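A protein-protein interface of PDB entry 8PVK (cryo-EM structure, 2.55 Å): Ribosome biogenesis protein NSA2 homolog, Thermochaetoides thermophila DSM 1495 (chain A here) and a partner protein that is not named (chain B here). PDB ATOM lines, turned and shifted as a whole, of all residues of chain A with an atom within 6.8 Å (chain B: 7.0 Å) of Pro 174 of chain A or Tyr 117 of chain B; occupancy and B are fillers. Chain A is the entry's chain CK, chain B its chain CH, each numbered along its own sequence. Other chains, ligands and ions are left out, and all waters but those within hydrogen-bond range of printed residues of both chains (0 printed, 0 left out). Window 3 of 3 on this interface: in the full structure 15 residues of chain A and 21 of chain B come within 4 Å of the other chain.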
ATOM      1  N   ILE A 150      22.462 -21.556 -24.913  1.00  0.00           N
ATOM      2  CA  ILE A 150      21.665 -20.358 -24.668  1.00  0.00           C
ATOM      3  C   ILE A 150      20.361 -20.468 -25.451  1.00  0.00           C
ATOM      4  O   ILE A 150      20.364 -20.819 -26.637  1.00  0.00           O
ATOM      5  CB  ILE A 150      22.443 -19.074 -25.021  1.00  0.00           C
ATOM      6  CG1 ILE A 150      21.576 -17.830 -24.809  1.00  0.00           C
ATOM      7  CG2 ILE A 150      23.018 -19.118 -26.434  1.00  0.00           C
ATOM      8  CD1 ILE A 150      22.356 -16.541 -24.829  1.00  0.00           C
ATOM      9  N   VAL A 151      19.244 -20.204 -24.779  1.00  0.00           N
ATOM     10  CA  VAL A 151      17.935 -20.253 -25.420  1.00  0.00           C
ATOM     11  C   VAL A 151      17.734 -18.966 -26.211  1.00  0.00           C
ATOM     12  O   VAL A 151      17.820 -17.865 -25.657  1.00  0.00           O
ATOM     13  CB  VAL A 151      16.818 -20.451 -24.387  1.00  0.00           C
ATOM     14  CG1 VAL A 151      15.491 -20.693 -25.082  1.00  0.00           C
ATOM     15  CG2 VAL A 151      17.157 -21.603 -23.457  1.00  0.00           C
ATOM     16  N   THR A 152      17.463 -19.101 -27.508  1.00  0.00           N
ATOM     17  CA  THR A 152      17.375 -17.967 -28.417  1.00  0.00           C
ATOM     18  C   THR A 152      15.950 -17.474 -28.637  1.00  0.00           C
ATOM     19  O   THR A 152      15.746 -16.551 -29.430  1.00  0.00           O
ATOM     20  CB  THR A 152      18.003 -18.326 -29.769  1.00  0.00           C
ATOM     21  OG1 THR A 152      17.198 -19.312 -30.424  1.00  0.00           O
ATOM     22  CG2 THR A 152      19.406 -18.874 -29.574  1.00  0.00           C
ATOM     23  N   LYS A 153      14.971 -18.057 -27.960  1.00  0.00           N
ATOM     24  CA  LYS A 153      13.570 -17.688 -28.076  1.00  0.00           C
ATOM     25  C   LYS A 153      13.069 -17.149 -26.741  1.00  0.00           C
ATOM     26  O   LYS A 153      13.692 -17.389 -25.700  1.00  0.00           O
ATOM     27  CB  LYS A 153      12.730 -18.899 -28.514  1.00  0.00           C
ATOM     28  CG  LYS A 153      13.272 -19.621 -29.732  1.00  0.00           C
ATOM     29  CD  LYS A 153      12.862 -18.958 -31.029  1.00  0.00           C
ATOM     30  CE  LYS A 153      13.279 -19.808 -32.217  1.00  0.00           C
ATOM     31  NZ  LYS A 153      12.859 -19.211 -33.512  1.00  0.00           N
ATOM     32  N   THR A 155      11.209 -16.787 -23.243  1.00  0.00           N
ATOM     33  CA  THR A 155      10.894 -17.773 -22.221  1.00  0.00           C
ATOM     34  C   THR A 155      10.090 -17.130 -21.099  1.00  0.00           C
ATOM     35  O   THR A 155      10.083 -15.910 -20.925  1.00  0.00           O
ATOM     36  CB  THR A 155      12.159 -18.419 -21.620  1.00  0.00           C
ATOM     37  OG1 THR A 155      12.934 -17.424 -20.941  1.00  0.00           O
ATOM     38  CG2 THR A 155      13.008 -19.085 -22.693  1.00  0.00           C
ATOM     39  N   VAL A 157       9.923 -17.673 -16.998  1.00  0.00           N
ATOM     40  CA  VAL A 157      10.685 -18.328 -15.937  1.00  0.00           C
ATOM     41  C   VAL A 157       9.879 -18.552 -14.665  1.00  0.00           C
ATOM     42  O   VAL A 157      10.325 -19.315 -13.793  1.00  0.00           O
ATOM     43  CB  VAL A 157      11.972 -17.541 -15.603  1.00  0.00           C
ATOM     44  CG1 VAL A 157      12.838 -17.397 -16.841  1.00  0.00           C
ATOM     45  CG2 VAL A 157      11.636 -16.183 -15.020  1.00  0.00           C
ATOM     46  N   GLU A 169      25.180 -23.694 -14.534  1.00  0.00           N
ATOM     47  CA  GLU A 169      24.113 -23.160 -15.381  1.00  0.00           C
ATOM     48  C   GLU A 169      24.382 -23.607 -16.814  1.00  0.00           C
ATOM     49  O   GLU A 169      25.090 -22.943 -17.570  1.00  0.00           O
ATOM     50  CB  GLU A 169      24.034 -21.642 -15.274  1.00  0.00           C
ATOM     51  CG  GLU A 169      22.839 -21.042 -15.998  1.00  0.00           C
ATOM     52  CD  GLU A 169      23.057 -19.597 -16.396  1.00  0.00           C
ATOM     53  OE1 GLU A 169      24.198 -19.105 -16.269  1.00  0.00           O
ATOM     54  OE2 GLU A 169      22.088 -18.953 -16.846  1.00  0.00           O
ATOM     55  N   ILE A 172      21.030 -21.195 -20.520  1.00  0.00           N
ATOM     56  CA  ILE A 172      21.032 -19.764 -20.259  1.00  0.00           C
ATOM     57  C   ILE A 172      19.767 -19.169 -20.854  1.00  0.00           C
ATOM     58  O   ILE A 172      19.577 -19.183 -22.076  1.00  0.00           O
ATOM     59  CB  ILE A 172      22.283 -19.091 -20.846  1.00  0.00           C
ATOM     60  CG1 ILE A 172      23.550 -19.683 -20.223  1.00  0.00           C
ATOM     61  CG2 ILE A 172      22.222 -17.586 -20.651  1.00  0.00           C
ATOM     62  CD1 ILE A 172      24.805 -19.385 -21.006  1.00  0.00           C
ATOM     63  N   ARG A 173      18.906 -18.638 -19.992  1.00  0.00           N
ATOM     64  CA  ARG A 173      17.711 -17.922 -20.425  1.00  0.00           C
ATOM     65  C   ARG A 173      17.900 -16.454 -20.081  1.00  0.00           C
ATOM     66  O   ARG A 173      17.697 -16.059 -18.923  1.00  0.00           O
ATOM     67  CB  ARG A 173      16.460 -18.485 -19.747  1.00  0.00           C
ATOM     68  CG  ARG A 173      16.139 -19.914 -20.151  1.00  0.00           C
ATOM     69  CD  ARG A 173      14.955 -20.463 -19.380  1.00  0.00           C
ATOM     70  NE  ARG A 173      15.311 -20.802 -18.009  1.00  0.00           N
ATOM     71  CZ  ARG A 173      14.463 -21.285 -17.111  1.00  0.00           C
ATOM     72  NH1 ARG A 173      13.193 -21.501 -17.407  1.00  0.00           N
ATOM     73  NH2 ARG A 173      14.901 -21.557 -15.885  1.00  0.00           N
ATOM     74  N   PRO A 174      18.305 -15.614 -21.037  1.00  0.00           N
ATOM     75  CA  PRO A 174      18.677 -14.235 -20.707  1.00  0.00           C
ATOM     76  C   PRO A 174      17.494 -13.402 -20.239  1.00  0.00           C
ATOM     77  O   PRO A 174      16.345 -13.642 -20.618  1.00  0.00           O
ATOM     78  CB  PRO A 174      19.246 -13.693 -22.023  1.00  0.00           C
ATOM     79  CG  PRO A 174      18.730 -14.600 -23.076  1.00  0.00           C
ATOM     80  CD  PRO A 174      18.574 -15.941 -22.446  1.00  0.00           C
ATOM     81  N   MET A 175      17.800 -12.412 -19.395  1.00  0.00           N
ATOM     82  CA  MET A 175      16.760 -11.579 -18.799  1.00  0.00           C
ATOM     83  C   MET A 175      16.058 -10.717 -19.838  1.00  0.00           C
ATOM     84  O   MET A 175      14.893 -10.351 -19.649  1.00  0.00           O
ATOM     85  CB  MET A 175      17.348 -10.686 -17.709  1.00  0.00           C
ATOM     86  CG  MET A 175      18.340 -11.369 -16.793  1.00  0.00           C
ATOM     87  SD  MET A 175      18.963 -10.237 -15.536  1.00  0.00           S
ATOM     88  CE  MET A 175      20.537  -9.757 -16.241  1.00  0.00           C
ATOM     89  N   GLY A 176      16.747 -10.373 -20.927  1.00  0.00           N
ATOM     90  CA  GLY A 176      16.133  -9.574 -21.969  1.00  0.00           C
ATOM     91  C   GLY A 176      15.079 -10.306 -22.770  1.00  0.00           C
ATOM     92  O   GLY A 176      14.259  -9.660 -23.428  1.00  0.00           O
ATOM     93  N   LEU A 177      15.075 -11.639 -22.722  1.00  0.00           N
ATOM     94  CA  LEU A 177      14.119 -12.449 -23.465  1.00  0.00           C
ATOM     95  C   LEU A 177      13.031 -13.042 -22.575  1.00  0.00           C
ATOM     96  O   LEU A 177      12.327 -13.961 -22.998  1.00  0.00           O
ATOM     97  CB  LEU A 177      14.847 -13.562 -24.220  1.00  0.00           C
ATOM     98  CG  LEU A 177      15.463 -13.207 -25.574  1.00  0.00           C
ATOM     99  CD1 LEU A 177      16.444 -14.277 -26.014  1.00  0.00           C
ATOM    100  CD2 LEU A 177      14.378 -13.020 -26.619  1.00  0.00           C
ATOM    101  N   ARG A 178      12.876 -12.543 -21.353  1.00  0.00           N
ATOM    102  CA  ARG A 178      11.866 -13.048 -20.433  1.00  0.00           C
ATOM    103  C   ARG A 178      10.608 -12.194 -20.519  1.00  0.00           C
ATOM    104  O   ARG A 178      10.682 -10.962 -20.466  1.00  0.00           O
ATOM    105  CB  ARG A 178      12.390 -13.072 -18.997  1.00  0.00           C
ATOM    106  CG  ARG A 178      13.549 -14.021 -18.776  1.00  0.00           C
ATOM    107  CD  ARG A 178      14.096 -13.898 -17.369  1.00  0.00           C
ATOM    108  NE  ARG A 178      15.422 -14.488 -17.250  1.00  0.00           N
ATOM    109  CZ  ARG A 178      16.201 -14.371 -16.184  1.00  0.00           C
ATOM    110  NH1 ARG A 178      15.809 -13.706 -15.111  1.00  0.00           N
ATOM    111  NH2 ARG A 178      17.404 -14.936 -16.196  1.00  0.00           N
ATOM    112  N   ARG B  42      23.226  -7.225 -36.713  1.00  0.00           N
ATOM    113  CA  ARG B  42      22.675  -6.658 -35.486  1.00  0.00           C
ATOM    114  C   ARG B  42      23.009  -5.180 -35.362  1.00  0.00           C
ATOM    115  O   ARG B  42      22.159  -4.381 -34.958  1.00  0.00           O
ATOM    116  CB  ARG B  42      23.204  -7.415 -34.269  1.00  0.00           C
ATOM    117  CG  ARG B  42      22.605  -8.788 -34.041  1.00  0.00           C
ATOM    118  CD  ARG B  42      23.377  -9.512 -32.952  1.00  0.00           C
ATOM    119  NE  ARG B  42      22.993 -10.912 -32.824  1.00  0.00           N
ATOM    120  CZ  ARG B  42      23.688 -11.814 -32.147  1.00  0.00           C
ATOM    121  NH1 ARG B  42      24.814 -11.499 -31.530  1.00  0.00           N
ATOM    122  NH2 ARG B  42      23.240 -13.065 -32.084  1.00  0.00           N
ATOM    123  N   VAL B 112      16.111  -2.787 -29.016  1.00  0.00           N
ATOM    124  CA  VAL B 112      17.568  -2.908 -29.034  1.00  0.00           C
ATOM    125  C   VAL B 112      18.009  -4.092 -28.176  1.00  0.00           C
ATOM    126  O   VAL B 112      18.904  -4.864 -28.562  1.00  0.00           O
ATOM    127  CB  VAL B 112      18.214  -1.583 -28.585  1.00  0.00           C
ATOM    128  CG1 VAL B 112      19.658  -1.782 -28.154  1.00  0.00           C
ATOM    129  CG2 VAL B 112      18.149  -0.567 -29.713  1.00  0.00           C
ATOM    130  N   ARG B 113      17.356  -4.282 -27.024  1.00  0.00           N
ATOM    131  CA  ARG B 113      17.657  -5.436 -26.181  1.00  0.00           C
ATOM    132  C   ARG B 113      17.336  -6.751 -26.888  1.00  0.00           C
ATOM    133  O   ARG B 113      18.056  -7.743 -26.724  1.00  0.00           O
ATOM    134  CB  ARG B 113      16.889  -5.327 -24.867  1.00  0.00           C
ATOM    135  CG  ARG B 113      17.433  -6.194 -23.751  1.00  0.00           C
ATOM    136  CD  ARG B 113      16.702  -5.921 -22.450  1.00  0.00           C
ATOM    137  NE  ARG B 113      16.783  -4.520 -22.055  1.00  0.00           N
ATOM    138  CZ  ARG B 113      15.741  -3.704 -21.970  1.00  0.00           C
ATOM    139  NH1 ARG B 113      14.518  -4.114 -22.264  1.00  0.00           N
ATOM    140  NH2 ARG B 113      15.931  -2.447 -21.584  1.00  0.00           N
ATOM    141  N   LEU B 114      16.256  -6.782 -27.674  1.00  0.00           N
ATOM    142  CA  LEU B 114      15.930  -7.995 -28.428  1.00  0.00           C
ATOM    143  C   LEU B 114      16.888  -8.211 -29.599  1.00  0.00           C
ATOM    144  O   LEU B 114      17.250  -9.355 -29.917  1.00  0.00           O
ATOM    145  CB  LEU B 114      14.488  -7.935 -28.923  1.00  0.00           C
ATOM    146  CG  LEU B 114      13.428  -7.898 -27.825  1.00  0.00           C
ATOM    147  CD1 LEU B 114      12.055  -7.686 -28.424  1.00  0.00           C
ATOM    148  CD2 LEU B 114      13.472  -9.169 -26.992  1.00  0.00           C
ATOM    149  N   LEU B 115      17.300  -7.126 -30.261  1.00  0.00           N
ATOM    150  CA  LEU B 115      18.269  -7.218 -31.344  1.00  0.00           C
ATOM    151  C   LEU B 115      19.636  -7.670 -30.855  1.00  0.00           C
ATOM    152  O   LEU B 115      20.427  -8.173 -31.658  1.00  0.00           O
ATOM    153  CB  LEU B 115      18.388  -5.871 -32.056  1.00  0.00           C
ATOM    154  CG  LEU B 115      17.341  -5.613 -33.139  1.00  0.00           C
ATOM    155  CD1 LEU B 115      17.471  -4.211 -33.706  1.00  0.00           C
ATOM    156  CD2 LEU B 115      17.459  -6.646 -34.237  1.00  0.00           C
ATOM    157  N   LYS B 116      19.931  -7.482 -29.565  1.00  0.00           N
ATOM    158  CA  LYS B 116      21.138  -8.075 -28.989  1.00  0.00           C
ATOM    159  C   LYS B 116      21.133  -9.598 -29.087  1.00  0.00           C
ATOM    160  O   LYS B 116      22.198 -10.213 -29.210  1.00  0.00           O
ATOM    161  CB  LYS B 116      21.292  -7.670 -27.524  1.00  0.00           C
ATOM    162  CG  LYS B 116      21.699  -6.230 -27.286  1.00  0.00           C
ATOM    163  CD  LYS B 116      22.364  -6.061 -25.921  1.00  0.00           C
ATOM    164  CE  LYS B 116      21.646  -6.845 -24.827  1.00  0.00           C
ATOM    165  NZ  LYS B 116      22.370  -6.784 -23.531  1.00  0.00           N
ATOM    166  N   TYR B 117      19.957 -10.222 -29.032  1.00  0.00           N
ATOM    167  CA  TYR B 117      19.844 -11.674 -28.998  1.00  0.00           C
ATOM    168  C   TYR B 117      19.278 -12.278 -30.274  1.00  0.00           C
ATOM    169  O   TYR B 117      19.149 -13.505 -30.348  1.00  0.00           O
ATOM    170  CB  TYR B 117      18.978 -12.107 -27.810  1.00  0.00           C
ATOM    171  CG  TYR B 117      19.556 -11.742 -26.466  1.00  0.00           C
ATOM    172  CD1 TYR B 117      20.653 -12.423 -25.955  1.00  0.00           C
ATOM    173  CD2 TYR B 117      19.004 -10.721 -25.706  1.00  0.00           C
ATOM    174  CE1 TYR B 117      21.186 -12.094 -24.728  1.00  0.00           C
ATOM    175  CE2 TYR B 117      19.530 -10.385 -24.476  1.00  0.00           C
ATOM    176  CZ  TYR B 117      20.621 -11.075 -23.992  1.00  0.00           C
ATOM    177  OH  TYR B 117      21.148 -10.744 -22.767  1.00  0.00           O
ATOM    178  N   ALA B 118      18.912 -11.464 -31.265  1.00  0.00           N
ATOM    179  CA  ALA B 118      18.454 -12.012 -32.538  1.00  0.00           C
ATOM    180  C   ALA B 118      19.575 -12.782 -33.237  1.00  0.00           C
ATOM    181  O   ALA B 118      20.761 -12.495 -33.063  1.00  0.00           O
ATOM    182  CB  ALA B 118      17.934 -10.898 -33.442  1.00  0.00           C
ATOM    183  N   GLN B 119      19.186 -13.778 -34.041  1.00  0.00           N
ATOM    184  CA  GLN B 119      20.126 -14.756 -34.577  1.00  0.00           C
ATOM    185  C   GLN B 119      20.210 -14.800 -36.098  1.00  0.00           C
ATOM    186  O   GLN B 119      21.025 -15.564 -36.627  1.00  0.00           O
ATOM    187  CB  GLN B 119      19.774 -16.162 -34.068  1.00  0.00           C
ATOM    188  CG  GLN B 119      19.912 -16.349 -32.567  1.00  0.00           C
ATOM    189  CD  GLN B 119      21.358 -16.394 -32.119  1.00  0.00           C
ATOM    190  OE1 GLN B 119      22.230 -16.869 -32.844  1.00  0.00           O
ATOM    191  NE2 GLN B 119      21.619 -15.897 -30.918  1.00  0.00           N
ATOM    192  N   SER B 120      19.408 -14.020 -36.819  1.00  0.00           N
ATOM    193  CA  SER B 120      19.444 -14.056 -38.274  1.00  0.00           C
ATOM    194  C   SER B 120      18.975 -12.717 -38.821  1.00  0.00           C
ATOM    195  O   SER B 120      18.390 -11.898 -38.105  1.00  0.00           O
ATOM    196  CB  SER B 120      18.586 -15.197 -38.833  1.00  0.00           C
ATOM    197  OG  SER B 120      17.221 -15.025 -38.499  1.00  0.00           O
ATOM    198  N   GLN B 123      15.062 -12.445 -38.658  1.00  0.00           N
ATOM    199  CA  GLN B 123      14.561 -12.094 -37.332  1.00  0.00           C
ATOM    200  C   GLN B 123      14.918 -10.657 -36.969  1.00  0.00           C
ATOM    201  O   GLN B 123      14.101  -9.936 -36.380  1.00  0.00           O
ATOM    202  CB  GLN B 123      15.114 -13.075 -36.298  1.00  0.00           C
ATOM    203  CG  GLN B 123      14.661 -12.815 -34.875  1.00  0.00           C
ATOM    204  CD  GLN B 123      15.446 -13.619 -33.863  1.00  0.00           C
ATOM    205  OE1 GLN B 123      16.363 -14.358 -34.218  1.00  0.00           O
ATOM    206  NE2 GLN B 123      15.094 -13.477 -32.592  1.00  0.00           N
ATOM    207  N   CYS B 124      16.130 -10.222 -37.332  1.00  0.00           N
ATOM    208  CA  CYS B 124      16.539  -8.837 -37.111  1.00  0.00           C
ATOM    209  C   CYS B 124      15.649  -7.862 -37.876  1.00  0.00           C
ATOM    210  O   CYS B 124      15.239  -6.825 -37.337  1.00  0.00           O
ATOM    211  CB  CYS B 124      17.997  -8.663 -37.534  1.00  0.00           C
ATOM    212  SG  CYS B 124      19.241  -9.105 -36.310  1.00  0.00           S
ATOM    213  N   LEU B 127      12.204  -7.690 -36.212  1.00  0.00           N
ATOM    214  CA  LEU B 127      12.235  -6.888 -34.990  1.00  0.00           C
ATOM    215  C   LEU B 127      12.345  -5.397 -35.296  1.00  0.00           C
ATOM    216  O   LEU B 127      11.699  -4.571 -34.633  1.00  0.00           O
ATOM    217  CB  LEU B 127      13.385  -7.345 -34.095  1.00  0.00           C
ATOM    218  CG  LEU B 127      13.199  -8.709 -33.429  1.00  0.00           C
ATOM    219  CD1 LEU B 127      14.486  -9.162 -32.761  1.00  0.00           C
ATOM    220  CD2 LEU B 127      12.056  -8.666 -32.429  1.00  0.00           C
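Gln 119 of chain B touches Thr 152 of chain A.
CB of Pro 174 of chain A touches CZ of Tyr 117 of chain B (3.6 Å).
Gly 176 of chain A touches Arg 113 of chain B.
Gly 176 of chain A touches Leu 114 of chain B.
CD2 of Leu 177 of chain A touches CD2 of Leu 114 of chain B, at 3.97 Å.
Leu 177 of chain A touches Tyr 117 of chain B.
The guanidinium group (NH2) of Arg 42 of chain B sits close to the side-chain amide nitrogen (NE2) of Gln 119 of chain B, 3.5 Å away.
The backbone NH of Gln 119 of chain B sits at hydrogen-bond distance from the side-chain amide oxygen of Gln 123 of chain B (2.9 Å).
The backbone NH (N) of Thr 155 of chain A is in hydrogen-bond range of the backbone carbonyl oxygen (O) of Leu 177 of chain A, at 3.0 Å.
The backbone carbonyl oxygen of Tyr 117 of chain B sits at hydrogen-bond distance from the side-chain amide nitrogen of Gln 119 of chain B (3.5 Å).
Of the 13 printed residues of chain B, 4 touch a printed residue of chain A.
Printed residues of chain B that touch a printed residue of chain A: Arg 113, Leu 114, Tyr 117 and Gln 119.
Hydrophobic or aromatic side chains of chain B that line the printed part of chain A: Leu 114 and Tyr 117.
Of the 14 printed residues of chain A, 4 touch a printed residue of chain B.
Hydrophobic or aromatic side chains of chain A that line the printed part of chain B: Pro 174 and Leu 177.
Among the printed residues, 6 pairs touch across the chains.
Arg 173 of chain A touches none of the printed residues of chain B.
Of chain B, only Tyr 117 (3.6 Å) comes within 4 Å of Pro 174 of chain A.
Of the printed residues of chain B, Gly 176 of chain A touches Arg 113 (3.7 Å) and Leu 114 (3.7 Å).
Printed residues of chain A within 4 Å of Gln 119 of chain B: Thr 152.
Cys 124 of chain B touches none of the printed residues of chain A.
The nearest printed residue of chain B that does not touch Pro 174 of chain A is Arg 113 of chain B (7.7 Å).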
